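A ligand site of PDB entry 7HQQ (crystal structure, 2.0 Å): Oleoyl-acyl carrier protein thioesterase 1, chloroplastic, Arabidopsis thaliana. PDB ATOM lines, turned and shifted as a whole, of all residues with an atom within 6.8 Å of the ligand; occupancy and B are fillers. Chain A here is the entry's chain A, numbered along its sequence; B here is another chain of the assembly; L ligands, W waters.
The side-chain carboxylate (OE1) of Glu 31 sits at hydrogen-bond distance from a nitrogen (N1) of the ligand.
A nitrogen (N2) of the ligand sits at hydrogen-bond distance from the backbone NH of Val 30, 3.0 Å away.
An oxygen (O1) of the ligand lies within hydrogen-bond range of the guanidinium group of Arg 185 of chain B (3.0 Å).
O of Leu 204 sits close to O1 of the ligand, at 3.4 Å.
The side-chain carboxylate (OE2) of Glu 31 is in salt-bridge range of the guanidinium group (NH1) of Arg 184 of chain B (3.9 Å).
The backbone carbonyl oxygen of Leu 204 sits at hydrogen-bond distance from the guanidinium group of Arg 185 of chain B, 3.2 Å away.
The backbone NH (N) of Arg 185 of chain B lies within hydrogen-bond range of the side-chain carboxylate (OE1) of Glu 205 (2.9 Å).
The guanidinium group (NH2) of Arg 185 of chain B sits at hydrogen-bond distance from the backbone carbonyl oxygen (O) of Ile 207, at 2.9 Å.
N of Thr 32 lies within hydrogen-bond range of OG1 of Thr 29, 3.2 Å away.
CB of Thr 29 touches N2 of the ligand, at 3.6 Å.
Val 212 touches the ligand (CG2 to C6, 3.8 Å).
Trp 283 touches the ligand.
Within 4 Å of the ligand: Thr 29, Val 30, Glu 31, Leu 204, Val 212, Trp 283 and Arg 185 of chain B.
Water W1 lies within hydrogen-bond range of OE1 of Glu 205, O of Gly 201 and O1 of the ligand.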
ATOM      1  N   ASN A  25       4.509 -18.870 -18.254  1.00  0.00           N
ATOM      2  CA  ASN A  25       5.964 -19.092 -18.220  1.00  0.00           C
ATOM      3  C   ASN A  25       6.499 -19.725 -19.524  1.00  0.00           C
ATOM      4  O   ASN A  25       7.692 -20.052 -19.586  1.00  0.00           O
ATOM      5  CB  ASN A  25       6.325 -19.994 -17.022  1.00  0.00           C
ATOM      6  CG  ASN A  25       6.051 -19.402 -15.663  1.00  0.00           C
ATOM      7  OD1 ASN A  25       5.888 -20.127 -14.675  1.00  0.00           O
ATOM      8  ND2 ASN A  25       6.005 -18.074 -15.560  1.00  0.00           N
ATOM      9  N   ALA A  28       4.669 -26.028 -19.700  1.00  0.00           N
ATOM     10  CA  ALA A  28       3.489 -26.791 -19.314  1.00  0.00           C
ATOM     11  C   ALA A  28       3.013 -26.454 -17.908  1.00  0.00           C
ATOM     12  O   ALA A  28       3.819 -26.403 -16.988  1.00  0.00           O
ATOM     13  CB  ALA A  28       3.784 -28.276 -19.420  1.00  0.00           C
ATOM     14  N   THR A  29       1.721 -26.196 -17.743  1.00  0.00           N
ATOM     15  CA  THR A  29       1.147 -25.916 -16.445  1.00  0.00           C
ATOM     16  C   THR A  29       1.172 -27.169 -15.549  1.00  0.00           C
ATOM     17  O   THR A  29       1.352 -28.283 -16.057  1.00  0.00           O
ATOM     18  CB  THR A  29      -0.286 -25.397 -16.622  1.00  0.00           C
ATOM     19  OG1 THR A  29      -1.067 -26.407 -17.275  1.00  0.00           O
ATOM     20  CG2 THR A  29      -0.343 -24.091 -17.430  1.00  0.00           C
ATOM     21  N   VAL A  30       0.944 -27.009 -14.227  1.00  0.00           N
ATOM     22  CA  VAL A  30       0.876 -28.176 -13.341  1.00  0.00           C
ATOM     23  C   VAL A  30      -0.374 -29.028 -13.673  1.00  0.00           C
ATOM     24  O   VAL A  30      -0.321 -30.240 -13.557  1.00  0.00           O
ATOM     25  CB  VAL A  30       1.019 -27.836 -11.835  1.00  0.00           C
ATOM     26  CG1 VAL A  30      -0.298 -27.388 -11.234  1.00  0.00           C
ATOM     27  CG2 VAL A  30       1.600 -29.024 -11.082  1.00  0.00           C
ATOM     28  N   GLU A  31      -1.453 -28.404 -14.187  1.00  0.00           N
ATOM     29  CA  GLU A  31      -2.670 -29.095 -14.596  1.00  0.00           C
ATOM     30  C   GLU A  31      -2.410 -29.943 -15.834  1.00  0.00           C
ATOM     31  O   GLU A  31      -2.965 -31.026 -15.932  1.00  0.00           O
ATOM     32  CB  GLU A  31      -3.810 -28.107 -14.854  1.00  0.00           C
ATOM     33  CG  GLU A  31      -4.210 -27.340 -13.606  1.00  0.00           C
ATOM     34  CD  GLU A  31      -3.939 -25.839 -13.659  1.00  0.00           C
ATOM     35  OE1 GLU A  31      -2.965 -25.412 -14.322  1.00  0.00           O
ATOM     36  OE2 GLU A  31      -4.716 -25.102 -13.007  1.00  0.00           O
ATOM     37  N   THR A  32      -1.535 -29.479 -16.755  1.00  0.00           N
ATOM     38  CA  THR A  32      -1.165 -30.292 -17.912  1.00  0.00           C
ATOM     39  C   THR A  32      -0.379 -31.524 -17.427  1.00  0.00           C
ATOM     40  O   THR A  32      -0.684 -32.637 -17.859  1.00  0.00           O
ATOM     41  CB  THR A  32      -0.390 -29.474 -18.961  1.00  0.00           C
ATOM     42  OG1 THR A  32      -1.334 -28.652 -19.636  1.00  0.00           O
ATOM     43  CG2 THR A  32       0.335 -30.386 -19.992  1.00  0.00           C
ATOM     44  N   TYR A  80       9.836 -27.708 -15.593  1.00  0.00           N
ATOM     45  CA  TYR A  80       8.654 -27.879 -16.424  1.00  0.00           C
ATOM     46  C   TYR A  80       9.058 -27.956 -17.896  1.00  0.00           C
ATOM     47  O   TYR A  80       9.841 -27.121 -18.361  1.00  0.00           O
ATOM     48  CB  TYR A  80       7.695 -26.700 -16.230  1.00  0.00           C
ATOM     49  CG  TYR A  80       6.925 -26.730 -14.937  1.00  0.00           C
ATOM     50  CD1 TYR A  80       7.408 -26.098 -13.797  1.00  0.00           C
ATOM     51  CD2 TYR A  80       5.699 -27.391 -14.845  1.00  0.00           C
ATOM     52  CE1 TYR A  80       6.668 -26.082 -12.619  1.00  0.00           C
ATOM     53  CE2 TYR A  80       4.951 -27.367 -13.683  1.00  0.00           C
ATOM     54  CZ  TYR A  80       5.436 -26.717 -12.560  1.00  0.00           C
ATOM     55  OH  TYR A  80       4.733 -26.745 -11.385  1.00  0.00           O
ATOM     56  N   ILE A 200      -6.992 -29.195  -8.327  1.00  0.00           N
ATOM     57  CA  ILE A 200      -5.666 -28.567  -8.304  1.00  0.00           C
ATOM     58  C   ILE A 200      -5.800 -27.123  -8.806  1.00  0.00           C
ATOM     59  O   ILE A 200      -5.281 -26.208  -8.196  1.00  0.00           O
ATOM     60  CB  ILE A 200      -4.652 -29.387  -9.161  1.00  0.00           C
ATOM     61  CG1 ILE A 200      -4.353 -30.778  -8.526  1.00  0.00           C
ATOM     62  CG2 ILE A 200      -3.361 -28.578  -9.413  1.00  0.00           C
ATOM     63  CD1 ILE A 200      -3.550 -31.721  -9.417  1.00  0.00           C
ATOM     64  N   GLY A 201      -6.517 -26.942  -9.907  1.00  0.00           N
ATOM     65  CA  GLY A 201      -6.763 -25.618 -10.467  1.00  0.00           C
ATOM     66  C   GLY A 201      -7.460 -24.695  -9.493  1.00  0.00           C
ATOM     67  O   GLY A 201      -7.014 -23.556  -9.278  1.00  0.00           O
ATOM     68  N   VAL A 203      -7.598 -25.034  -6.074  1.00  0.00           N
ATOM     69  CA  VAL A 203      -6.695 -24.739  -4.948  1.00  0.00           C
ATOM     70  C   VAL A 203      -5.767 -23.543  -5.314  1.00  0.00           C
ATOM     71  O   VAL A 203      -5.605 -22.579  -4.527  1.00  0.00           O
ATOM     72  CB  VAL A 203      -5.857 -26.003  -4.577  1.00  0.00           C
ATOM     73  CG1 VAL A 203      -4.573 -25.659  -3.815  1.00  0.00           C
ATOM     74  CG2 VAL A 203      -6.684 -27.002  -3.788  1.00  0.00           C
ATOM     75  N   LEU A 204      -5.134 -23.614  -6.498  1.00  0.00           N
ATOM     76  CA  LEU A 204      -4.192 -22.599  -6.952  1.00  0.00           C
ATOM     77  C   LEU A 204      -4.834 -21.236  -7.281  1.00  0.00           C
ATOM     78  O   LEU A 204      -4.128 -20.231  -7.283  1.00  0.00           O
ATOM     79  CB  LEU A 204      -3.358 -23.122  -8.129  1.00  0.00           C
ATOM     80  CG  LEU A 204      -2.566 -24.413  -7.866  1.00  0.00           C
ATOM     81  CD1 LEU A 204      -1.971 -24.966  -9.140  1.00  0.00           C
ATOM     82  CD2 LEU A 204      -1.503 -24.211  -6.779  1.00  0.00           C
ATOM     83  N   GLU A 205      -6.166 -21.183  -7.503  1.00  0.00           N
ATOM     84  CA  GLU A 205      -6.894 -19.952  -7.788  1.00  0.00           C
ATOM     85  C   GLU A 205      -6.723 -18.911  -6.693  1.00  0.00           C
ATOM     86  O   GLU A 205      -6.742 -17.726  -7.007  1.00  0.00           O
ATOM     87  CB  GLU A 205      -8.408 -20.202  -7.956  1.00  0.00           C
ATOM     88  CG  GLU A 205      -8.865 -20.478  -9.384  1.00  0.00           C
ATOM     89  CD  GLU A 205      -8.434 -19.453 -10.431  1.00  0.00           C
ATOM     90  OE1 GLU A 205      -7.465 -19.742 -11.172  1.00  0.00           O
ATOM     91  OE2 GLU A 205      -9.091 -18.400 -10.531  1.00  0.00           O
ATOM     92  N   SER A 206      -6.596 -19.319  -5.419  1.00  0.00           N
ATOM     93  CA  SER A 206      -6.441 -18.370  -4.334  1.00  0.00           C
ATOM     94  C   SER A 206      -4.985 -17.927  -4.073  1.00  0.00           C
ATOM     95  O   SER A 206      -4.766 -17.111  -3.200  1.00  0.00           O
ATOM     96  CB  SER A 206      -7.117 -18.857  -3.052  1.00  0.00           C
ATOM     97  OG  SER A 206      -6.668 -20.164  -2.697  1.00  0.00           O
ATOM     98  N   ILE A 207      -4.003 -18.414  -4.861  1.00  0.00           N
ATOM     99  CA  ILE A 207      -2.628 -17.928  -4.769  1.00  0.00           C
ATOM    100  C   ILE A 207      -2.645 -16.541  -5.440  1.00  0.00           C
ATOM    101  O   ILE A 207      -3.209 -16.415  -6.535  1.00  0.00           O
ATOM    102  CB  ILE A 207      -1.665 -18.882  -5.528  1.00  0.00           C
ATOM    103  CG1 ILE A 207      -1.554 -20.261  -4.841  1.00  0.00           C
ATOM    104  CG2 ILE A 207      -0.273 -18.226  -5.767  1.00  0.00           C
ATOM    105  CD1 ILE A 207      -0.607 -20.364  -3.627  1.00  0.00           C
ATOM    106  N   VAL A 212       2.391 -15.886  -8.438  1.00  0.00           N
ATOM    107  CA  VAL A 212       2.417 -16.555  -9.755  1.00  0.00           C
ATOM    108  C   VAL A 212       3.439 -15.919 -10.721  1.00  0.00           C
ATOM    109  O   VAL A 212       4.181 -16.633 -11.394  1.00  0.00           O
ATOM    110  CB  VAL A 212       0.987 -16.662 -10.360  1.00  0.00           C
ATOM    111  CG1 VAL A 212       1.013 -17.341 -11.730  1.00  0.00           C
ATOM    112  CG2 VAL A 212       0.043 -17.401  -9.420  1.00  0.00           C
ATOM    113  N   LEU A 217       5.724 -22.950  -9.114  1.00  0.00           N
ATOM    114  CA  LEU A 217       5.231 -23.979  -8.205  1.00  0.00           C
ATOM    115  C   LEU A 217       6.178 -25.182  -8.259  1.00  0.00           C
ATOM    116  O   LEU A 217       6.385 -25.752  -9.321  1.00  0.00           O
ATOM    117  CB  LEU A 217       3.822 -24.411  -8.630  1.00  0.00           C
ATOM    118  CG  LEU A 217       3.213 -25.557  -7.836  1.00  0.00           C
ATOM    119  CD1 LEU A 217       2.888 -25.110  -6.432  1.00  0.00           C
ATOM    120  CD2 LEU A 217       1.949 -26.054  -8.496  1.00  0.00           C
ATOM    121  N   TRP A 283       6.773 -22.891  -3.350  1.00  0.00           N
ATOM    122  CA  TRP A 283       7.120 -22.170  -4.565  1.00  0.00           C
ATOM    123  C   TRP A 283       8.539 -21.619  -4.454  1.00  0.00           C
ATOM    124  O   TRP A 283       8.915 -21.120  -3.393  1.00  0.00           O
ATOM    125  CB  TRP A 283       6.156 -20.977  -4.772  1.00  0.00           C
ATOM    126  CG  TRP A 283       4.701 -21.337  -4.815  1.00  0.00           C
ATOM    127  CD1 TRP A 283       3.959 -21.877  -3.814  1.00  0.00           C
ATOM    128  CD2 TRP A 283       3.817 -21.155  -5.917  1.00  0.00           C
ATOM    129  NE1 TRP A 283       2.678 -22.081  -4.237  1.00  0.00           N
ATOM    130  CE2 TRP A 283       2.553 -21.646  -5.523  1.00  0.00           C
ATOM    131  CE3 TRP A 283       3.966 -20.648  -7.213  1.00  0.00           C
ATOM    132  CZ2 TRP A 283       1.450 -21.639  -6.376  1.00  0.00           C
ATOM    133  CZ3 TRP A 283       2.876 -20.653  -8.065  1.00  0.00           C
ATOM    134  CH2 TRP A 283       1.638 -21.148  -7.638  1.00  0.00           C
ATOM    135  N   ARG B 184     -10.655 -19.458 -15.011  1.00  0.00           N
ATOM    136  CA  ARG B 184      -9.583 -19.705 -14.046  1.00  0.00           C
ATOM    137  C   ARG B 184      -8.213 -19.584 -14.769  1.00  0.00           C
ATOM    138  O   ARG B 184      -8.204 -19.350 -15.984  1.00  0.00           O
ATOM    139  CB  ARG B 184      -9.785 -21.009 -13.251  1.00  0.00           C
ATOM    140  CG  ARG B 184     -10.039 -22.247 -14.068  1.00  0.00           C
ATOM    141  CD  ARG B 184     -10.482 -23.321 -13.084  1.00  0.00           C
ATOM    142  NE  ARG B 184     -10.752 -24.607 -13.731  1.00  0.00           N
ATOM    143  CZ  ARG B 184      -9.853 -25.545 -13.944  1.00  0.00           C
ATOM    144  NH1 ARG B 184      -8.572 -25.344 -13.619  1.00  0.00           N
ATOM    145  NH2 ARG B 184     -10.200 -26.699 -14.506  1.00  0.00           N
ATOM    146  N   ARG B 185      -7.094 -19.687 -14.052  1.00  0.00           N
ATOM    147  CA  ARG B 185      -5.774 -19.517 -14.703  1.00  0.00           C
ATOM    148  C   ARG B 185      -5.518 -20.543 -15.826  1.00  0.00           C
ATOM    149  O   ARG B 185      -4.901 -20.178 -16.830  1.00  0.00           O
ATOM    150  CB  ARG B 185      -4.637 -19.474 -13.688  1.00  0.00           C
ATOM    151  CG  ARG B 185      -4.693 -18.234 -12.799  1.00  0.00           C
ATOM    152  CD  ARG B 185      -3.322 -17.879 -12.233  1.00  0.00           C
ATOM    153  NE  ARG B 185      -3.392 -16.713 -11.347  1.00  0.00           N
ATOM    154  CZ  ARG B 185      -3.524 -16.779 -10.018  1.00  0.00           C
ATOM    155  NH1 ARG B 185      -3.596 -17.959  -9.414  1.00  0.00           N
ATOM    156  NH2 ARG B 185      -3.589 -15.671  -9.305  1.00  0.00           N
ATOM    157  N   ALA B 186      -6.071 -21.778 -15.716  1.00  0.00           N
ATOM    158  CA  ALA B 186      -5.948 -22.775 -16.807  1.00  0.00           C
ATOM    159  C   ALA B 186      -6.715 -22.357 -18.078  1.00  0.00           C
ATOM    160  O   ALA B 186      -6.418 -22.857 -19.142  1.00  0.00           O
ATOM    161  CB  ALA B 186      -6.426 -24.139 -16.346  1.00  0.00           C
HETATM  162  C1  LIG L   1      -2.338 -22.380 -11.956  1.00  0.00           C
HETATM  163  C2  LIG L   1      -1.133 -22.998 -12.312  1.00  0.00           C
HETATM  164  N1  LIG L   1      -0.866 -24.036 -13.120  1.00  0.00           N
HETATM  165  N2  LIG L   1       0.474 -24.251 -13.241  1.00  0.00           N
HETATM  166  C3  LIG L   1       1.059 -23.393 -12.426  1.00  0.00           C
HETATM  167  C4  LIG L   1       0.097 -22.559 -11.794  1.00  0.00           C
HETATM  168  C5  LIG L   1       0.128 -21.479 -10.900  1.00  0.00           C
HETATM  169  C6  LIG L   1      -1.052 -20.893 -10.524  1.00  0.00           C
HETATM  170  C7  LIG L   1      -2.284 -21.359 -11.029  1.00  0.00           C
HETATM  171  O1  LIG L   1      -3.418 -20.748 -10.591  1.00  0.00           O
HETATM  172  O   HOH W   1      -5.906 -21.783 -10.851  1.00  0.00           O
